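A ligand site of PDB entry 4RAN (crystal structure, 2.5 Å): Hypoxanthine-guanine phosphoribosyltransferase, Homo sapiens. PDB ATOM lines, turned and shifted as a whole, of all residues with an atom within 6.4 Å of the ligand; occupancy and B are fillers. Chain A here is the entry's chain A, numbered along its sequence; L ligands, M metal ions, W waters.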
ATOM      1  N   LEU A 101      -6.930  30.512 -23.223  1.00  0.00           N
ATOM      2  CA  LEU A 101      -6.259  30.597 -24.505  1.00  0.00           C
ATOM      3  C   LEU A 101      -6.539  29.408 -25.433  1.00  0.00           C
ATOM      4  O   LEU A 101      -6.668  28.274 -24.963  1.00  0.00           O
ATOM      5  CB  LEU A 101      -4.752  30.797 -24.314  1.00  0.00           C
ATOM      6  CG  LEU A 101      -4.413  32.095 -23.576  1.00  0.00           C
ATOM      7  CD1 LEU A 101      -2.907  32.266 -23.437  1.00  0.00           C
ATOM      8  CD2 LEU A 101      -5.019  33.284 -24.299  1.00  0.00           C
ATOM      9  N   LYS A 102      -6.613  29.689 -26.727  1.00  0.00           N
ATOM     10  CA  LYS A 102      -6.904  28.684 -27.743  1.00  0.00           C
ATOM     11  C   LYS A 102      -5.915  27.520 -27.709  1.00  0.00           C
ATOM     12  O   LYS A 102      -5.449  27.062 -28.754  1.00  0.00           O
ATOM     13  CB  LYS A 102      -6.907  29.329 -29.129  1.00  0.00           C
ATOM     14  N   GLU A 133       0.187  31.519 -14.524  1.00  0.00           N
ATOM     15  CA  GLU A 133       0.061  30.362 -15.409  1.00  0.00           C
ATOM     16  C   GLU A 133       0.438  29.085 -14.679  1.00  0.00           C
ATOM     17  O   GLU A 133       1.195  29.116 -13.706  1.00  0.00           O
ATOM     18  CB  GLU A 133       0.948  30.573 -16.646  1.00  0.00           C
ATOM     19  CG  GLU A 133       1.058  29.390 -17.600  1.00  0.00           C
ATOM     20  CD  GLU A 133      -0.178  29.179 -18.449  1.00  0.00           C
ATOM     21  OE1 GLU A 133      -1.228  28.796 -17.898  1.00  0.00           O
ATOM     22  OE2 GLU A 133      -0.092  29.381 -19.684  1.00  0.00           O
ATOM     23  N   ASP A 134      -0.079  27.943 -15.138  1.00  0.00           N
ATOM     24  CA  ASP A 134       0.253  26.659 -14.525  1.00  0.00           C
ATOM     25  C   ASP A 134       1.606  26.121 -14.964  1.00  0.00           C
ATOM     26  O   ASP A 134       2.400  25.671 -14.131  1.00  0.00           O
ATOM     27  CB  ASP A 134      -0.871  25.635 -14.773  1.00  0.00           C
ATOM     28  CG  ASP A 134      -1.156  25.422 -16.253  1.00  0.00           C
ATOM     29  OD1 ASP A 134      -0.621  26.170 -17.096  1.00  0.00           O
ATOM     30  OD2 ASP A 134      -1.934  24.493 -16.570  1.00  0.00           O
ATOM     31  N   ILE A 135       1.889  26.166 -16.264  1.00  0.00           N
ATOM     32  CA  ILE A 135       3.147  25.598 -16.764  1.00  0.00           C
ATOM     33  C   ILE A 135       3.629  26.180 -18.101  1.00  0.00           C
ATOM     34  O   ILE A 135       2.874  26.278 -19.060  1.00  0.00           O
ATOM     35  CB  ILE A 135       3.078  24.054 -16.851  1.00  0.00           C
ATOM     36  CG1 ILE A 135       4.386  23.479 -17.396  1.00  0.00           C
ATOM     37  CG2 ILE A 135       1.885  23.618 -17.700  1.00  0.00           C
ATOM     38  CD1 ILE A 135       4.506  21.975 -17.241  1.00  0.00           C
ATOM     39  N   ILE A 136       4.910  26.570 -18.138  1.00  0.00           N
ATOM     40  CA  ILE A 136       5.583  26.948 -19.372  1.00  0.00           C
ATOM     41  C   ILE A 136       6.270  25.724 -19.953  1.00  0.00           C
ATOM     42  O   ILE A 136       7.044  25.059 -19.270  1.00  0.00           O
ATOM     43  CB  ILE A 136       6.660  28.024 -19.121  1.00  0.00           C
ATOM     44  CG1 ILE A 136       6.111  29.171 -18.280  1.00  0.00           C
ATOM     45  CG2 ILE A 136       7.236  28.518 -20.454  1.00  0.00           C
ATOM     46  CD1 ILE A 136       4.987  29.934 -18.932  1.00  0.00           C
ATOM     47  N   ASP A 137       5.997  25.419 -21.223  1.00  0.00           N
ATOM     48  CA  ASP A 137       6.668  24.314 -21.898  1.00  0.00           C
ATOM     49  C   ASP A 137       7.508  24.810 -23.077  1.00  0.00           C
ATOM     50  O   ASP A 137       8.711  25.028 -22.933  1.00  0.00           O
ATOM     51  CB  ASP A 137       5.664  23.249 -22.347  1.00  0.00           C
ATOM     52  CG  ASP A 137       6.324  21.975 -22.839  1.00  0.00           C
ATOM     53  OD1 ASP A 137       7.539  21.814 -22.607  1.00  0.00           O
ATOM     54  OD2 ASP A 137       5.632  21.127 -23.438  1.00  0.00           O
ATOM     55  N   THR A 138       6.871  24.991 -24.234  1.00  0.00           N
ATOM     56  CA  THR A 138       7.575  25.515 -25.398  1.00  0.00           C
ATOM     57  C   THR A 138       7.771  27.026 -25.298  1.00  0.00           C
ATOM     58  O   THR A 138       8.710  27.581 -25.864  1.00  0.00           O
ATOM     59  CB  THR A 138       6.861  25.188 -26.722  1.00  0.00           C
ATOM     60  OG1 THR A 138       5.648  25.949 -26.798  1.00  0.00           O
ATOM     61  CG2 THR A 138       6.543  23.703 -26.802  1.00  0.00           C
ATOM     62  N   GLY A 139       6.873  27.684 -24.564  1.00  0.00           N
ATOM     63  CA  GLY A 139       6.935  29.126 -24.375  1.00  0.00           C
ATOM     64  C   GLY A 139       5.993  29.895 -25.288  1.00  0.00           C
ATOM     65  O   GLY A 139       5.794  31.091 -25.118  1.00  0.00           O
ATOM     66  N   LYS A 140       5.421  29.189 -26.258  1.00  0.00           N
ATOM     67  CA  LYS A 140       4.551  29.834 -27.248  1.00  0.00           C
ATOM     68  C   LYS A 140       3.316  30.496 -26.625  1.00  0.00           C
ATOM     69  O   LYS A 140       3.013  31.649 -26.932  1.00  0.00           O
ATOM     70  CB  LYS A 140       4.127  28.827 -28.317  1.00  0.00           C
ATOM     71  CG  LYS A 140       5.276  28.303 -29.161  1.00  0.00           C
ATOM     72  CD  LYS A 140       4.823  27.160 -30.069  1.00  0.00           C
ATOM     73  CE  LYS A 140       6.014  26.491 -30.748  1.00  0.00           C
ATOM     74  NZ  LYS A 140       6.798  27.451 -31.571  1.00  0.00           N
ATOM     75  N   THR A 141       2.622  29.764 -25.748  1.00  0.00           N
ATOM     76  CA  THR A 141       1.426  30.271 -25.087  1.00  0.00           C
ATOM     77  C   THR A 141       1.680  31.601 -24.398  1.00  0.00           C
ATOM     78  O   THR A 141       0.889  32.539 -24.519  1.00  0.00           O
ATOM     79  CB  THR A 141       0.894  29.254 -24.045  1.00  0.00           C
ATOM     80  OG1 THR A 141       0.407  28.094 -24.717  1.00  0.00           O
ATOM     81  CG2 THR A 141      -0.228  29.866 -23.234  1.00  0.00           C
ATOM     82  N   MET A 142       2.782  31.684 -23.666  1.00  0.00           N
ATOM     83  CA  MET A 142       3.111  32.900 -22.927  1.00  0.00           C
ATOM     84  C   MET A 142       3.558  34.030 -23.852  1.00  0.00           C
ATOM     85  O   MET A 142       3.194  35.194 -23.644  1.00  0.00           O
ATOM     86  CB  MET A 142       4.169  32.604 -21.862  1.00  0.00           C
ATOM     87  CG  MET A 142       4.263  33.658 -20.774  1.00  0.00           C
ATOM     88  SD  MET A 142       2.650  34.044 -20.068  1.00  0.00           S
ATOM     89  CE  MET A 142       2.138  32.432 -19.479  1.00  0.00           C
ATOM     90  N   LYS A 165       9.119  23.739 -17.590  1.00  0.00           N
ATOM     91  CA  LYS A 165       9.706  22.501 -18.073  1.00  0.00           C
ATOM     92  C   LYS A 165      11.085  22.709 -18.683  1.00  0.00           C
ATOM     93  O   LYS A 165      11.326  23.694 -19.367  1.00  0.00           O
ATOM     94  CB  LYS A 165       8.780  21.832 -19.090  1.00  0.00           C
ATOM     95  CG  LYS A 165       8.297  20.461 -18.669  1.00  0.00           C
ATOM     96  CD  LYS A 165       7.237  19.928 -19.617  1.00  0.00           C
ATOM     97  CE  LYS A 165       6.544  18.722 -19.021  1.00  0.00           C
ATOM     98  NZ  LYS A 165       5.469  18.185 -19.900  1.00  0.00           N
ATOM     99  N   ARG A 169      12.690  21.888 -26.812  1.00  0.00           N
ATOM    100  CA  ARG A 169      11.680  22.532 -27.651  1.00  0.00           C
ATOM    101  C   ARG A 169      11.416  23.970 -27.221  1.00  0.00           C
ATOM    102  O   ARG A 169      10.733  24.720 -27.924  1.00  0.00           O
ATOM    103  CB  ARG A 169      10.369  21.760 -27.630  1.00  0.00           C
ATOM    104  CG  ARG A 169      10.511  20.271 -27.792  1.00  0.00           C
ATOM    105  CD  ARG A 169       9.303  19.672 -28.492  1.00  0.00           C
ATOM    106  NE  ARG A 169       8.034  20.216 -28.034  1.00  0.00           N
ATOM    107  CZ  ARG A 169       7.434  19.874 -26.898  1.00  0.00           C
ATOM    108  NH1 ARG A 169       8.000  18.988 -26.086  1.00  0.00           N
ATOM    109  NH2 ARG A 169       6.273  20.423 -26.560  1.00  0.00           N
ATOM    110  N   ILE A 182      10.962  21.507 -13.728  1.00  0.00           N
ATOM    111  CA  ILE A 182      10.790  20.053 -13.785  1.00  0.00           C
ATOM    112  C   ILE A 182      11.325  19.456 -15.090  1.00  0.00           C
ATOM    113  O   ILE A 182      11.520  20.177 -16.071  1.00  0.00           O
ATOM    114  CB  ILE A 182       9.298  19.673 -13.626  1.00  0.00           C
ATOM    115  CG1 ILE A 182       8.492  20.142 -14.830  1.00  0.00           C
ATOM    116  CG2 ILE A 182       8.743  20.243 -12.336  1.00  0.00           C
ATOM    117  CD1 ILE A 182       7.084  19.572 -14.877  1.00  0.00           C
ATOM    118  N   ASP A 184      11.158  16.904 -18.543  1.00  0.00           N
ATOM    119  CA  ASP A 184      10.138  16.773 -19.573  1.00  0.00           C
ATOM    120  C   ASP A 184       9.297  15.527 -19.340  1.00  0.00           C
ATOM    121  O   ASP A 184       9.408  14.540 -20.069  1.00  0.00           O
ATOM    122  CB  ASP A 184      10.783  16.719 -20.961  1.00  0.00           C
ATOM    123  CG  ASP A 184       9.800  17.080 -22.072  1.00  0.00           C
ATOM    124  OD1 ASP A 184       8.582  17.020 -21.839  1.00  0.00           O
ATOM    125  OD2 ASP A 184      10.270  17.409 -23.180  1.00  0.00           O
ATOM    126  N   LYS A 185       8.453  15.570 -18.310  1.00  0.00           N
ATOM    127  CA  LYS A 185       7.503  14.496 -18.029  1.00  0.00           C
ATOM    128  C   LYS A 185       6.101  15.070 -17.933  1.00  0.00           C
ATOM    129  O   LYS A 185       5.909  16.152 -17.387  1.00  0.00           O
ATOM    130  CB  LYS A 185       7.861  13.783 -16.725  1.00  0.00           C
ATOM    131  CG  LYS A 185       9.116  12.929 -16.807  1.00  0.00           C
ATOM    132  CD  LYS A 185       9.388  12.234 -15.484  1.00  0.00           C
ATOM    133  CE  LYS A 185      10.612  11.338 -15.557  1.00  0.00           C
ATOM    134  NZ  LYS A 185      10.923  10.687 -14.246  1.00  0.00           N
ATOM    135  N   PHE A 186       5.108  14.357 -18.460  1.00  0.00           N
ATOM    136  CA  PHE A 186       3.743  14.877 -18.449  1.00  0.00           C
ATOM    137  C   PHE A 186       3.089  14.753 -17.071  1.00  0.00           C
ATOM    138  O   PHE A 186       2.793  13.655 -16.603  1.00  0.00           O
ATOM    139  CB  PHE A 186       2.877  14.204 -19.514  1.00  0.00           C
ATOM    140  CG  PHE A 186       1.582  14.911 -19.774  1.00  0.00           C
ATOM    141  CD1 PHE A 186       1.511  15.922 -20.709  1.00  0.00           C
ATOM    142  CD2 PHE A 186       0.447  14.591 -19.055  1.00  0.00           C
ATOM    143  CE1 PHE A 186       0.325  16.591 -20.949  1.00  0.00           C
ATOM    144  CE2 PHE A 186      -0.744  15.263 -19.278  1.00  0.00           C
ATOM    145  CZ  PHE A 186      -0.805  16.258 -20.227  1.00  0.00           C
ATOM    146  N   VAL A 187       2.860  15.897 -16.435  1.00  0.00           N
ATOM    147  CA  VAL A 187       2.293  15.932 -15.087  1.00  0.00           C
ATOM    148  C   VAL A 187       0.834  16.374 -15.089  1.00  0.00           C
ATOM    149  O   VAL A 187       0.392  17.082 -15.998  1.00  0.00           O
ATOM    150  CB  VAL A 187       3.093  16.863 -14.166  1.00  0.00           C
ATOM    151  CG1 VAL A 187       4.470  16.287 -13.886  1.00  0.00           C
ATOM    152  CG2 VAL A 187       3.199  18.256 -14.779  1.00  0.00           C
ATOM    153  N   VAL A 188       0.093  15.962 -14.073  1.00  0.00           N
ATOM    154  CA  VAL A 188      -1.302  16.347 -13.902  1.00  0.00           C
ATOM    155  C   VAL A 188      -1.570  16.697 -12.447  1.00  0.00           C
ATOM    156  O   VAL A 188      -0.693  16.556 -11.603  1.00  0.00           O
ATOM    157  CB  VAL A 188      -2.264  15.232 -14.338  1.00  0.00           C
ATOM    158  CG1 VAL A 188      -2.203  15.022 -15.845  1.00  0.00           C
ATOM    159  CG2 VAL A 188      -1.958  13.945 -13.599  1.00  0.00           C
ATOM    160  N   LEU A 192      -3.909  21.082 -13.229  1.00  0.00           N
ATOM    161  CA  LEU A 192      -3.358  20.593 -14.500  1.00  0.00           C
ATOM    162  C   LEU A 192      -4.093  19.316 -14.906  1.00  0.00           C
ATOM    163  O   LEU A 192      -4.474  18.523 -14.046  1.00  0.00           O
ATOM    164  CB  LEU A 192      -1.847  20.334 -14.407  1.00  0.00           C
ATOM    165  CG  LEU A 192      -0.955  21.580 -14.405  1.00  0.00           C
ATOM    166  CD1 LEU A 192      -0.788  22.134 -12.999  1.00  0.00           C
ATOM    167  CD2 LEU A 192       0.401  21.269 -15.030  1.00  0.00           C
ATOM    168  N   ASP A 193      -4.286  19.122 -16.201  1.00  0.00           N
ATOM    169  CA  ASP A 193      -5.183  18.077 -16.675  1.00  0.00           C
ATOM    170  C   ASP A 193      -4.616  17.140 -17.732  1.00  0.00           C
ATOM    171  O   ASP A 193      -3.549  17.380 -18.290  1.00  0.00           O
ATOM    172  CB  ASP A 193      -6.469  18.701 -17.219  1.00  0.00           C
ATOM    173  CG  ASP A 193      -6.291  19.291 -18.609  1.00  0.00           C
ATOM    174  OD1 ASP A 193      -5.248  19.923 -18.866  1.00  0.00           O
ATOM    175  OD2 ASP A 193      -7.196  19.101 -19.455  1.00  0.00           O
ATOM    176  N   TYR A 194      -5.361  16.068 -17.990  1.00  0.00           N
ATOM    177  CA  TYR A 194      -5.132  15.212 -19.132  1.00  0.00           C
ATOM    178  C   TYR A 194      -6.487  14.925 -19.752  1.00  0.00           C
ATOM    179  O   TYR A 194      -7.257  14.125 -19.219  1.00  0.00           O
ATOM    180  CB  TYR A 194      -4.457  13.896 -18.713  1.00  0.00           C
ATOM    181  CG  TYR A 194      -4.284  12.924 -19.857  1.00  0.00           C
ATOM    182  CD1 TYR A 194      -3.278  13.098 -20.804  1.00  0.00           C
ATOM    183  CD2 TYR A 194      -5.121  11.828 -20.001  1.00  0.00           C
ATOM    184  CE1 TYR A 194      -3.114  12.218 -21.846  1.00  0.00           C
ATOM    185  CE2 TYR A 194      -4.965  10.937 -21.045  1.00  0.00           C
ATOM    186  CZ  TYR A 194      -3.965  11.131 -21.965  1.00  0.00           C
ATOM    187  OH  TYR A 194      -3.801  10.251 -23.008  1.00  0.00           O
HETATM  188  N1  LIG L   1      -2.038  25.705 -26.157  1.00  0.00           N
HETATM  189  C1  LIG L   1      -1.874  25.686 -24.892  1.00  0.00           C
HETATM  190  C2  LIG L   1      -1.671  25.670 -23.421  1.00  0.00           C
HETATM  191  C3  LIG L   1      -1.056  24.507 -22.766  1.00  0.00           C
HETATM  192  N2  LIG L   1       0.340  24.211 -22.954  1.00  0.00           N
HETATM  193  C4  LIG L   1       1.103  25.468 -22.987  1.00  0.00           C
HETATM  194  C5  LIG L   1       2.608  25.193 -22.699  1.00  0.00           C
HETATM  195  P1  LIG L   1       3.684  25.974 -23.976  1.00  0.00           P
HETATM  196  O1  LIG L   1       4.814  26.790 -23.285  1.00  0.00           O
HETATM  197  O2  LIG L   1       2.839  26.955 -24.910  1.00  0.00           O
HETATM  198  O3  LIG L   1       4.292  24.880 -24.823  1.00  0.00           O
HETATM  199  C6  LIG L   1       0.787  23.363 -21.831  1.00  0.00           C
HETATM  200  C7  LIG L   1       0.574  21.920 -22.225  1.00  0.00           C
HETATM  201  N3  LIG L   1       1.478  21.047 -21.481  1.00  0.00           N
HETATM  202  C8  LIG L   1       1.094  20.272 -20.424  1.00  0.00           C
HETATM  203  N4  LIG L   1      -0.085  20.101 -19.817  1.00  0.00           N
HETATM  204  C9  LIG L   1      -0.187  19.271 -18.793  1.00  0.00           C
HETATM  205  N5  LIG L   1      -1.438  19.089 -18.153  1.00  0.00           N
HETATM  206  N6  LIG L   1       0.913  18.582 -18.341  1.00  0.00           N
HETATM  207  C10 LIG L   1       2.119  18.719 -18.904  1.00  0.00           C
HETATM  208  O4  LIG L   1       3.215  17.994 -18.406  1.00  0.00           O
HETATM  209  C11 LIG L   1       2.248  19.590 -19.998  1.00  0.00           C
HETATM  210  N7  LIG L   1       3.293  19.998 -20.847  1.00  0.00           N
HETATM  211  C12 LIG L   1       2.810  20.894 -21.749  1.00  0.00           C
HETATM  212 MG    MG M   1      -1.694  27.434 -19.512  1.00  0.00          MG
HETATM  213  O   HOH W   1       4.393  29.175 -22.185  1.00  0.00           O
HETATM  214  O   HOH W   2       0.157  26.137 -20.089  1.00  0.00           O
HETATM  215  O   HOH W   3       3.558  22.270 -24.859  1.00  0.00           O
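O of Lys 185 sits close to O4 of the ligand, 3.4 Å away. Ile 135 touches the ligand (O to C5, 3.8 Å). C of Ile 136 touches O1 of the ligand, at 3.8 Å. Lys 140 touches the ligand (N to O2, 3.7 Å). Phe 186 touches the ligand (CA to O4, 3.2 Å). Leu 192 touches the ligand.
Water W1 bridges an oxygen (O1) of the ligand (2.7 Å) and the backbone NH (N) of Met 142 (3.3 Å). Water W3 lies within hydrogen-bond range of an oxygen (O3) of the ligand (2.7 Å) and the side-chain carboxylate of Asp 137 (2.8 Å). Water W2 lies within hydrogen-bond range of O of Ile 135 (2.9 Å) and OD1 of Asp 134 (3.1 Å).
The side-chain hydroxyl (OG1) of Thr 138 is in hydrogen-bond range of the backbone NH (N) of Lys 140. The side-chain amino group (NZ) of Lys 165 sits close to the backbone carbonyl oxygen (O) of Lys 185, 3.3 Å away. The backbone NH (N) of Lys 165 lies within hydrogen-bond range of the backbone carbonyl oxygen (O) of Ile 136 (3.0 Å). The side-chain amino group (NZ) of Lys 165 lies within salt-bridge range of the side-chain carboxylate (OD1) of Asp 184 (3.8 Å). The side-chain carboxylate (OD2) of Asp 137 is in salt-bridge range of the guanidinium group (NH2) of Arg 169 (3.3 Å).
The backbone NH of Gly 139 is in hydrogen-bond range of an oxygen (O1) of the ligand, 2.6 Å away. O3 of the ligand lies within hydrogen-bond range of N of Thr 138. The side-chain hydroxyl (OG1) of Thr 138 is in hydrogen-bond range of an oxygen (O3) of the ligand (2.6 Å). An oxygen (O2) of the ligand is in hydrogen-bond range of the backbone NH (N) of Thr 141 (2.9 Å). An oxygen (O2) of the ligand is in hydrogen-bond range of the side-chain hydroxyl of Thr 141 (2.7 Å). The side-chain amino group of Lys 165 is in hydrogen-bond range of an oxygen (O4) of the ligand. O of Asp 193 sits at hydrogen-bond distance from N5 of the ligand. N of Asp 137 lies within hydrogen-bond range of O1 of the ligand (2.7 Å). The backbone NH of Val 187 sits at hydrogen-bond distance from an oxygen (O4) of the ligand (2.9 Å). The backbone carbonyl oxygen of Val 187 is in hydrogen-bond range of a nitrogen (N6) of the ligand (2.8 Å).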
